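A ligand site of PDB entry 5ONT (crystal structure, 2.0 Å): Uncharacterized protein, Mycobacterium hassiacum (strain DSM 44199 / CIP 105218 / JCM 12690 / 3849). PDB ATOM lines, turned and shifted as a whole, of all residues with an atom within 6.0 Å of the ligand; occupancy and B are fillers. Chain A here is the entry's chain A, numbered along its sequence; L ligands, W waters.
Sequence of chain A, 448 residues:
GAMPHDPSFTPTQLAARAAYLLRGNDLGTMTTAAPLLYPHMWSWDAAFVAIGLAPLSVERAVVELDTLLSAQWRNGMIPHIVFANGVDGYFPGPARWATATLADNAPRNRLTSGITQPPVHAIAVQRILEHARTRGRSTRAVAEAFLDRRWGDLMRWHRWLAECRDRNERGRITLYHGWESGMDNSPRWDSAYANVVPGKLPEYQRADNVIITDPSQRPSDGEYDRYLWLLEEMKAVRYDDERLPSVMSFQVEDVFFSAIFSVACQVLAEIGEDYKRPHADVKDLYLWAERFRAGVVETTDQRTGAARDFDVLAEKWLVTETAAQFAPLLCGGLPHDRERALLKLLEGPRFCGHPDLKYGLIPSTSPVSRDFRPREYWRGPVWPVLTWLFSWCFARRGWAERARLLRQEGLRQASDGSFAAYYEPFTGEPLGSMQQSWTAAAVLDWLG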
ATOM      1  N   ALA A  33      28.599  17.029  -3.684  1.00  0.00           N
ATOM      2  CA  ALA A  33      28.328  17.625  -4.978  1.00  0.00           C
ATOM      3  C   ALA A  33      29.615  17.799  -5.761  1.00  0.00           C
ATOM      4  O   ALA A  33      29.664  17.553  -6.976  1.00  0.00           O
ATOM      5  CB  ALA A  33      27.605  18.977  -4.796  1.00  0.00           C
ATOM      6  N   ALA A  34      30.700  18.201  -5.073  1.00  0.00           N
ATOM      7  CA  ALA A  34      32.028  18.247  -5.659  1.00  0.00           C
ATOM      8  C   ALA A  34      33.009  18.186  -4.502  1.00  0.00           C
ATOM      9  O   ALA A  34      32.755  18.809  -3.461  1.00  0.00           O
ATOM     10  CB  ALA A  34      32.234  19.524  -6.496  1.00  0.00           C
ATOM     11  N   TYR A  38      32.168  21.945  -2.916  1.00  0.00           N
ATOM     12  CA  TYR A  38      30.833  21.657  -2.415  1.00  0.00           C
ATOM     13  C   TYR A  38      30.833  20.314  -1.688  1.00  0.00           C
ATOM     14  O   TYR A  38      30.200  19.358  -2.148  1.00  0.00           O
ATOM     15  CB  TYR A  38      29.830  21.666  -3.581  1.00  0.00           C
ATOM     16  CG  TYR A  38      29.880  22.907  -4.446  1.00  0.00           C
ATOM     17  CD1 TYR A  38      29.684  24.167  -3.892  1.00  0.00           C
ATOM     18  CD2 TYR A  38      30.101  22.828  -5.830  1.00  0.00           C
ATOM     19  CE1 TYR A  38      29.719  25.328  -4.660  1.00  0.00           C
ATOM     20  CE2 TYR A  38      30.139  23.994  -6.620  1.00  0.00           C
ATOM     21  CZ  TYR A  38      29.951  25.231  -6.023  1.00  0.00           C
ATOM     22  OH  TYR A  38      29.987  26.391  -6.750  1.00  0.00           O
ATOM     23  N   TRP A  42      24.011  18.353  -1.925  1.00  0.00           N
ATOM     24  CA  TRP A  42      23.079  19.346  -2.431  1.00  0.00           C
ATOM     25  C   TRP A  42      21.847  18.626  -2.973  1.00  0.00           C
ATOM     26  O   TRP A  42      21.963  17.562  -3.572  1.00  0.00           O
ATOM     27  CB  TRP A  42      23.698  20.213  -3.527  1.00  0.00           C
ATOM     28  CG  TRP A  42      24.231  21.563  -3.016  1.00  0.00           C
ATOM     29  CD1 TRP A  42      23.649  22.805  -3.181  1.00  0.00           C
ATOM     30  CD2 TRP A  42      25.450  21.784  -2.304  1.00  0.00           C
ATOM     31  NE1 TRP A  42      24.435  23.776  -2.587  1.00  0.00           N
ATOM     32  CE2 TRP A  42      25.540  23.165  -2.037  1.00  0.00           C
ATOM     33  CE3 TRP A  42      26.465  20.929  -1.824  1.00  0.00           C
ATOM     34  CZ2 TRP A  42      26.620  23.726  -1.341  1.00  0.00           C
ATOM     35  CZ3 TRP A  42      27.532  21.505  -1.117  1.00  0.00           C
ATOM     36  CH2 TRP A  42      27.604  22.884  -0.908  1.00  0.00           C
ATOM     37  N   SER A  43      20.677  19.234  -2.792  1.00  0.00           N
ATOM     38  CA  SER A  43      19.420  18.534  -3.075  1.00  0.00           C
ATOM     39  C   SER A  43      19.245  18.173  -4.551  1.00  0.00           C
ATOM     40  O   SER A  43      18.985  17.010  -4.872  1.00  0.00           O
ATOM     41  CB  SER A  43      18.237  19.367  -2.608  1.00  0.00           C
ATOM     42  OG  SER A  43      17.057  18.747  -3.122  1.00  0.00           O
ATOM     43  N   TRP A  44      19.287  19.155  -5.477  1.00  0.00           N
ATOM     44  CA  TRP A  44      19.020  18.672  -6.815  1.00  0.00           C
ATOM     45  C   TRP A  44      20.230  17.964  -7.419  1.00  0.00           C
ATOM     46  O   TRP A  44      20.031  17.053  -8.211  1.00  0.00           O
ATOM     47  CB  TRP A  44      18.405  19.736  -7.769  1.00  0.00           C
ATOM     48  CG  TRP A  44      19.212  20.904  -8.338  1.00  0.00           C
ATOM     49  CD1 TRP A  44      20.309  21.533  -7.769  1.00  0.00           C
ATOM     50  CD2 TRP A  44      18.956  21.588  -9.567  1.00  0.00           C
ATOM     51  NE1 TRP A  44      20.742  22.570  -8.590  1.00  0.00           N
ATOM     52  CE2 TRP A  44      19.930  22.620  -9.694  1.00  0.00           C
ATOM     53  CE3 TRP A  44      17.995  21.441 -10.584  1.00  0.00           C
ATOM     54  CZ2 TRP A  44      19.972  23.478 -10.797  1.00  0.00           C
ATOM     55  CZ3 TRP A  44      18.045  22.278 -11.685  1.00  0.00           C
ATOM     56  CH2 TRP A  44      19.032  23.294 -11.781  1.00  0.00           C
ATOM     57  N   ASP A  45      21.465  18.260  -6.948  1.00  0.00           N
ATOM     58  CA  ASP A  45      22.601  17.398  -7.289  1.00  0.00           C
ATOM     59  C   ASP A  45      22.357  15.964  -6.843  1.00  0.00           C
ATOM     60  O   ASP A  45      22.642  15.019  -7.594  1.00  0.00           O
ATOM     61  CB  ASP A  45      23.929  17.878  -6.667  1.00  0.00           C
ATOM     62  CG  ASP A  45      24.297  19.284  -7.070  1.00  0.00           C
ATOM     63  OD1 ASP A  45      23.456  20.162  -6.846  1.00  0.00           O
ATOM     64  OD2 ASP A  45      25.431  19.529  -7.579  1.00  0.00           O
ATOM     65  N   HIS A  80      18.130  22.501   0.667  1.00  0.00           N
ATOM     66  CA  HIS A  80      19.011  22.410  -0.496  1.00  0.00           C
ATOM     67  C   HIS A  80      20.403  21.887  -0.165  1.00  0.00           C
ATOM     68  O   HIS A  80      21.088  21.404  -1.068  1.00  0.00           O
ATOM     69  CB  HIS A  80      19.073  23.747  -1.244  1.00  0.00           C
ATOM     70  CG  HIS A  80      20.160  24.700  -0.814  1.00  0.00           C
ATOM     71  ND1 HIS A  80      20.282  25.175   0.479  1.00  0.00           N
ATOM     72  CD2 HIS A  80      21.109  25.347  -1.536  1.00  0.00           C
ATOM     73  CE1 HIS A  80      21.281  26.048   0.536  1.00  0.00           C
ATOM     74  NE2 HIS A  80      21.785  26.183  -0.675  1.00  0.00           N
ATOM     75  N   ILE A  81      20.825  21.949   1.106  1.00  0.00           N
ATOM     76  CA  ILE A  81      22.083  21.349   1.555  1.00  0.00           C
ATOM     77  C   ILE A  81      21.803  20.463   2.767  1.00  0.00           C
ATOM     78  O   ILE A  81      21.097  20.876   3.695  1.00  0.00           O
ATOM     79  CB  ILE A  81      23.148  22.399   1.923  1.00  0.00           C
ATOM     80  CG1 ILE A  81      23.399  23.369   0.765  1.00  0.00           C
ATOM     81  CG2 ILE A  81      24.504  21.685   2.331  1.00  0.00           C
ATOM     82  CD1 ILE A  81      24.313  24.503   1.188  1.00  0.00           C
ATOM     83  N   TYR A  90      33.020  24.762   3.583  1.00  0.00           N
ATOM     84  CA  TYR A  90      31.972  25.500   2.900  1.00  0.00           C
ATOM     85  C   TYR A  90      31.359  26.537   3.840  1.00  0.00           C
ATOM     86  O   TYR A  90      31.226  26.304   5.050  1.00  0.00           O
ATOM     87  CB  TYR A  90      30.883  24.567   2.354  1.00  0.00           C
ATOM     88  CG  TYR A  90      29.799  25.314   1.595  1.00  0.00           C
ATOM     89  CD1 TYR A  90      29.986  25.715   0.288  1.00  0.00           C
ATOM     90  CD2 TYR A  90      28.605  25.637   2.203  1.00  0.00           C
ATOM     91  CE1 TYR A  90      29.010  26.415  -0.402  1.00  0.00           C
ATOM     92  CE2 TYR A  90      27.623  26.344   1.524  1.00  0.00           C
ATOM     93  CZ  TYR A  90      27.831  26.740   0.214  1.00  0.00           C
ATOM     94  OH  TYR A  90      26.857  27.470  -0.461  1.00  0.00           O
ATOM     95  N   GLN A 117      15.195  23.768  -3.197  1.00  0.00           N
ATOM     96  CA  GLN A 117      15.849  23.656  -4.500  1.00  0.00           C
ATOM     97  C   GLN A 117      14.921  22.844  -5.432  1.00  0.00           C
ATOM     98  O   GLN A 117      13.971  22.206  -4.948  1.00  0.00           O
ATOM     99  CB  GLN A 117      17.253  23.008  -4.358  1.00  0.00           C
ATOM    100  CG  GLN A 117      18.406  23.969  -4.773  1.00  0.00           C
ATOM    101  CD  GLN A 117      19.782  23.228  -4.920  1.00  0.00           C
ATOM    102  OE1 GLN A 117      19.868  22.021  -4.743  1.00  0.00           O
ATOM    103  NE2 GLN A 117      20.824  23.960  -5.281  1.00  0.00           N
ATOM    104  N   TRP A 179      19.193  31.278  -4.492  1.00  0.00           N
ATOM    105  CA  TRP A 179      19.827  29.961  -4.376  1.00  0.00           C
ATOM    106  C   TRP A 179      18.816  28.846  -4.621  1.00  0.00           C
ATOM    107  O   TRP A 179      19.182  27.769  -5.120  1.00  0.00           O
ATOM    108  CB  TRP A 179      20.463  29.793  -3.007  1.00  0.00           C
ATOM    109  CG  TRP A 179      21.812  30.467  -2.849  1.00  0.00           C
ATOM    110  CD1 TRP A 179      22.642  30.891  -3.834  1.00  0.00           C
ATOM    111  CD2 TRP A 179      22.470  30.774  -1.617  1.00  0.00           C
ATOM    112  NE1 TRP A 179      23.786  31.439  -3.302  1.00  0.00           N
ATOM    113  CE2 TRP A 179      23.704  31.389  -1.933  1.00  0.00           C
ATOM    114  CE3 TRP A 179      22.135  30.611  -0.279  1.00  0.00           C
ATOM    115  CZ2 TRP A 179      24.602  31.840  -0.962  1.00  0.00           C
ATOM    116  CZ3 TRP A 179      23.028  31.057   0.705  1.00  0.00           C
ATOM    117  CH2 TRP A 179      24.250  31.658   0.352  1.00  0.00           C
ATOM    118  N   GLY A 182      18.388  27.230  -8.100  1.00  0.00           N
ATOM    119  CA  GLY A 182      19.529  26.518  -8.650  1.00  0.00           C
ATOM    120  C   GLY A 182      20.434  27.362  -9.527  1.00  0.00           C
ATOM    121  O   GLY A 182      21.548  26.935  -9.818  1.00  0.00           O
ATOM    122  N   MET A 183      20.017  28.572  -9.892  1.00  0.00           N
ATOM    123  CA  MET A 183      20.800  29.417 -10.809  1.00  0.00           C
ATOM    124  C   MET A 183      21.200  30.684 -10.066  1.00  0.00           C
ATOM    125  O   MET A 183      20.722  31.795 -10.395  1.00  0.00           O
ATOM    126  CB  MET A 183      20.007  29.720 -12.068  1.00  0.00           C
ATOM    127  CG  MET A 183      19.532  28.489 -12.823  1.00  0.00           C
ATOM    128  SD  MET A 183      18.818  28.881 -14.448  1.00  0.00           S
ATOM    129  CE  MET A 183      17.823  27.427 -14.716  1.00  0.00           C
ATOM    130  N   ASP A 184      22.101  30.529  -9.086  1.00  0.00           N
ATOM    131  CA  ASP A 184      22.380  31.593  -8.105  1.00  0.00           C
ATOM    132  C   ASP A 184      22.432  32.989  -8.737  1.00  0.00           C
ATOM    133  O   ASP A 184      21.748  33.910  -8.280  1.00  0.00           O
ATOM    134  CB  ASP A 184      23.706  31.322  -7.379  1.00  0.00           C
ATOM    135  CG  ASP A 184      23.863  29.880  -6.912  1.00  0.00           C
ATOM    136  OD1 ASP A 184      23.006  28.981  -7.217  1.00  0.00           O
ATOM    137  OD2 ASP A 184      24.861  29.666  -6.197  1.00  0.00           O
ATOM    138  N   TYR A 224      27.201  38.626  -2.850  1.00  0.00           N
ATOM    139  CA  TYR A 224      27.191  37.671  -1.748  1.00  0.00           C
ATOM    140  C   TYR A 224      26.607  38.277  -0.470  1.00  0.00           C
ATOM    141  O   TYR A 224      25.940  37.582   0.290  1.00  0.00           O
ATOM    142  CB  TYR A 224      28.610  37.138  -1.502  1.00  0.00           C
ATOM    143  CG  TYR A 224      28.648  35.636  -1.261  1.00  0.00           C
ATOM    144  CD1 TYR A 224      28.605  34.747  -2.331  1.00  0.00           C
ATOM    145  CD2 TYR A 224      28.693  35.119   0.032  1.00  0.00           C
ATOM    146  CE1 TYR A 224      28.611  33.390  -2.116  1.00  0.00           C
ATOM    147  CE2 TYR A 224      28.706  33.755   0.246  1.00  0.00           C
ATOM    148  CZ  TYR A 224      28.661  32.893  -0.827  1.00  0.00           C
ATOM    149  OH  TYR A 224      28.674  31.529  -0.613  1.00  0.00           O
ATOM    150  N   TRP A 378      26.009  31.174 -14.205  1.00  0.00           N
ATOM    151  CA  TRP A 378      24.758  31.036 -14.923  1.00  0.00           C
ATOM    152  C   TRP A 378      24.512  32.194 -15.887  1.00  0.00           C
ATOM    153  O   TRP A 378      23.419  32.312 -16.436  1.00  0.00           O
ATOM    154  CB  TRP A 378      23.596  30.900 -13.922  1.00  0.00           C
ATOM    155  CG  TRP A 378      23.636  29.598 -13.126  1.00  0.00           C
ATOM    156  CD1 TRP A 378      24.139  29.422 -11.855  1.00  0.00           C
ATOM    157  CD2 TRP A 378      23.176  28.307 -13.546  1.00  0.00           C
ATOM    158  NE1 TRP A 378      24.009  28.115 -11.469  1.00  0.00           N
ATOM    159  CE2 TRP A 378      23.422  27.398 -12.487  1.00  0.00           C
ATOM    160  CE3 TRP A 378      22.551  27.825 -14.716  1.00  0.00           C
ATOM    161  CZ2 TRP A 378      23.071  26.063 -12.560  1.00  0.00           C
ATOM    162  CZ3 TRP A 378      22.235  26.484 -14.795  1.00  0.00           C
ATOM    163  CH2 TRP A 378      22.492  25.614 -13.713  1.00  0.00           C
ATOM    164  N   TRP A 383      25.916  24.340 -19.081  1.00  0.00           N
ATOM    165  CA  TRP A 383      25.878  23.426 -17.928  1.00  0.00           C
ATOM    166  C   TRP A 383      25.387  22.059 -18.372  1.00  0.00           C
ATOM    167  O   TRP A 383      24.228  21.965 -18.817  1.00  0.00           O
ATOM    168  CB  TRP A 383      24.954  23.995 -16.861  1.00  0.00           C
ATOM    169  CG  TRP A 383      25.460  25.218 -16.172  1.00  0.00           C
ATOM    170  CD1 TRP A 383      25.606  26.475 -16.718  1.00  0.00           C
ATOM    171  CD2 TRP A 383      25.841  25.335 -14.800  1.00  0.00           C
ATOM    172  NE1 TRP A 383      26.100  27.347 -15.778  1.00  0.00           N
ATOM    173  CE2 TRP A 383      26.232  26.677 -14.591  1.00  0.00           C
ATOM    174  CE3 TRP A 383      25.919  24.432 -13.722  1.00  0.00           C
ATOM    175  CZ2 TRP A 383      26.668  27.143 -13.353  1.00  0.00           C
ATOM    176  CZ3 TRP A 383      26.359  24.903 -12.496  1.00  0.00           C
ATOM    177  CH2 TRP A 383      26.729  26.239 -12.323  1.00  0.00           C
ATOM    178  N   GLN A 436      32.630  17.364 -10.720  1.00  0.00           N
ATOM    179  CA  GLN A 436      31.256  17.618 -10.315  1.00  0.00           C
ATOM    180  C   GLN A 436      30.429  16.345 -10.496  1.00  0.00           C
ATOM    181  O   GLN A 436      30.282  15.849 -11.617  1.00  0.00           O
ATOM    182  CB  GLN A 436      30.693  18.777 -11.128  1.00  0.00           C
ATOM    183  CG  GLN A 436      29.424  19.379 -10.590  1.00  0.00           C
ATOM    184  CD  GLN A 436      29.646  20.279  -9.369  1.00  0.00           C
ATOM    185  OE1 GLN A 436      30.713  20.880  -9.200  1.00  0.00           O
ATOM    186  NE2 GLN A 436      28.644  20.356  -8.511  1.00  0.00           N
ATOM    187  N   TRP A 438      27.258  15.669 -10.540  1.00  0.00           N
ATOM    188  CA  TRP A 438      26.103  15.571 -11.426  1.00  0.00           C
ATOM    189  C   TRP A 438      26.498  15.584 -12.897  1.00  0.00           C
ATOM    190  O   TRP A 438      25.722  15.097 -13.721  1.00  0.00           O
ATOM    191  CB  TRP A 438      25.033  16.657 -11.151  1.00  0.00           C
ATOM    192  CG  TRP A 438      25.382  18.120 -11.333  1.00  0.00           C
ATOM    193  CD1 TRP A 438      26.521  18.653 -11.835  1.00  0.00           C
ATOM    194  CD2 TRP A 438      24.537  19.226 -10.968  1.00  0.00           C
ATOM    195  NE1 TRP A 438      26.438  20.050 -11.837  1.00  0.00           N
ATOM    196  CE2 TRP A 438      25.238  20.415 -11.285  1.00  0.00           C
ATOM    197  CE3 TRP A 438      23.251  19.319 -10.431  1.00  0.00           C
ATOM    198  CZ2 TRP A 438      24.700  21.700 -11.053  1.00  0.00           C
ATOM    199  CZ3 TRP A 438      22.711  20.603 -10.209  1.00  0.00           C
ATOM    200  CH2 TRP A 438      23.428  21.764 -10.525  1.00  0.00           C
HETATM  201  C1  LIG L   1      24.703  27.339  -3.781  1.00  0.00           C
HETATM  202  C2  LIG L   1      26.053  22.327  -6.019  1.00  0.00           C
HETATM  203  C3  LIG L   1      25.360  23.676  -6.335  1.00  0.00           C
HETATM  204  C4  LIG L   1      24.242  23.492  -7.389  1.00  0.00           C
HETATM  205  C5  LIG L   1      23.777  24.864  -7.903  1.00  0.00           C
HETATM  206  C6  LIG L   1      24.907  25.799  -8.290  1.00  0.00           C
HETATM  207  C7  LIG L   1      25.880  25.891  -7.104  1.00  0.00           C
HETATM  208  C8  LIG L   1      25.735  26.705  -4.745  1.00  0.00           C
HETATM  209  C9  LIG L   1      26.977  27.571  -4.854  1.00  0.00           C
HETATM  210  O1  LIG L   1      26.382  24.598  -6.762  1.00  0.00           O
HETATM  211  O2  LIG L   1      25.170  26.532  -6.034  1.00  0.00           O
HETATM  212  O3  LIG L   1      23.594  26.509  -3.527  1.00  0.00           O
HETATM  213  O4  LIG L   1      26.949  28.457  -3.781  1.00  0.00           O
HETATM  214  O5  LIG L   1      24.437  27.082  -8.616  1.00  0.00           O
HETATM  215  O6  LIG L   1      22.843  24.765  -8.953  1.00  0.00           O
HETATM  216  O7  LIG L   1      23.182  22.758  -6.778  1.00  0.00           O
HETATM  217  O8  LIG L   1      26.617  21.737  -7.172  1.00  0.00           O
HETATM  218  O   HOH W   1      27.860  23.681  -9.294  1.00  0.00           O
HETATM  219  O   HOH W   2      26.283  31.662  -4.958  1.00  0.00           O
HETATM  220  O   HOH W   3      21.707  26.996  -5.520  1.00  0.00           O
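The side-chain amide nitrogen (NE2) of Gln 436 is in hydrogen-bond range of an oxygen (O8) of the ligand (2.8 Å).
The indole nitrogen (NE1) of Trp 44 is in hydrogen-bond range of an oxygen (O7) of the ligand, at 3.0 Å.
An oxygen (O8) of the ligand lies within hydrogen-bond range of the side-chain carboxylate of Asp 45, 2.5 Å away.
An oxygen (O5) of the ligand is in hydrogen-bond range of the side-chain carboxylate (OD1) of Asp 184.
An oxygen (O7) of the ligand sits at hydrogen-bond distance from the side-chain amide nitrogen (NE2) of Gln 117 (3.0 Å).
The indole nitrogen (NE1) of Trp 378 is in hydrogen-bond range of an oxygen (O5) of the ligand (3.1 Å).
O of Gly 182 lies within hydrogen-bond range of O6 of the ligand (2.7 Å).
O3 of the ligand sits at hydrogen-bond distance from NE1 of Trp 42 (3.0 Å).
The side-chain hydroxyl (OH) of Tyr 90 sits at hydrogen-bond distance from an oxygen (O4) of the ligand, at 3.5 Å.
An oxygen (O3) of the ligand sits close to a ring nitrogen (NE2) of His 80, 3.4 Å away.
The side-chain amide nitrogen (NE2) of Gln 436 lies within hydrogen-bond range of the backbone carbonyl oxygen (O) of Ala 33, at 3.4 Å.
The side-chain amide oxygen of Gln 117 sits at hydrogen-bond distance from the backbone NH of Trp 44 (3.0 Å).
NE1 of Trp 378 sits at hydrogen-bond distance from O of Gly 182 (3.2 Å).
OE1 of Gln 117 lies within hydrogen-bond range of N of Ser 43 (3.5 Å).
O of Tyr 38 is in hydrogen-bond range of N of Ala 33.
The backbone carbonyl oxygen (O) of His 80 is in hydrogen-bond range of the backbone NH (N) of Ser 43 (2.8 Å).
NE2 of Gln 436 lies within hydrogen-bond range of OD2 of Asp 45, 3.4 Å away.
Merely in contact with the ligand: Ala 33, Tyr 38 and Trp 438.
Hydrophobic or aromatic side chains that line the ligand: Ala 33, Tyr 38, Trp 42, Trp 44, His 80, Trp 378 and Trp 438.
Within 4 Å of the ligand: Ala 33, Tyr 38, Trp 42, Trp 44, Asp 45, His 80, Tyr 90, Gln 117, Gly 182, Asp 184, Trp 378, Gln 436 and Trp 438.
Water W3 lies within hydrogen-bond range of O of Trp 179 (2.7 Å), O3 of the ligand (2.8 Å), OD1 of Asp 184 (2.9 Å) and NE2 of Gln 117 (3.2 Å).
Water W2 lies within hydrogen-bond range of the side-chain carboxylate of Asp 184 (2.7 Å), the indole nitrogen of Trp 179 (3.0 Å) and an oxygen (O4) of the ligand (3.5 Å).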
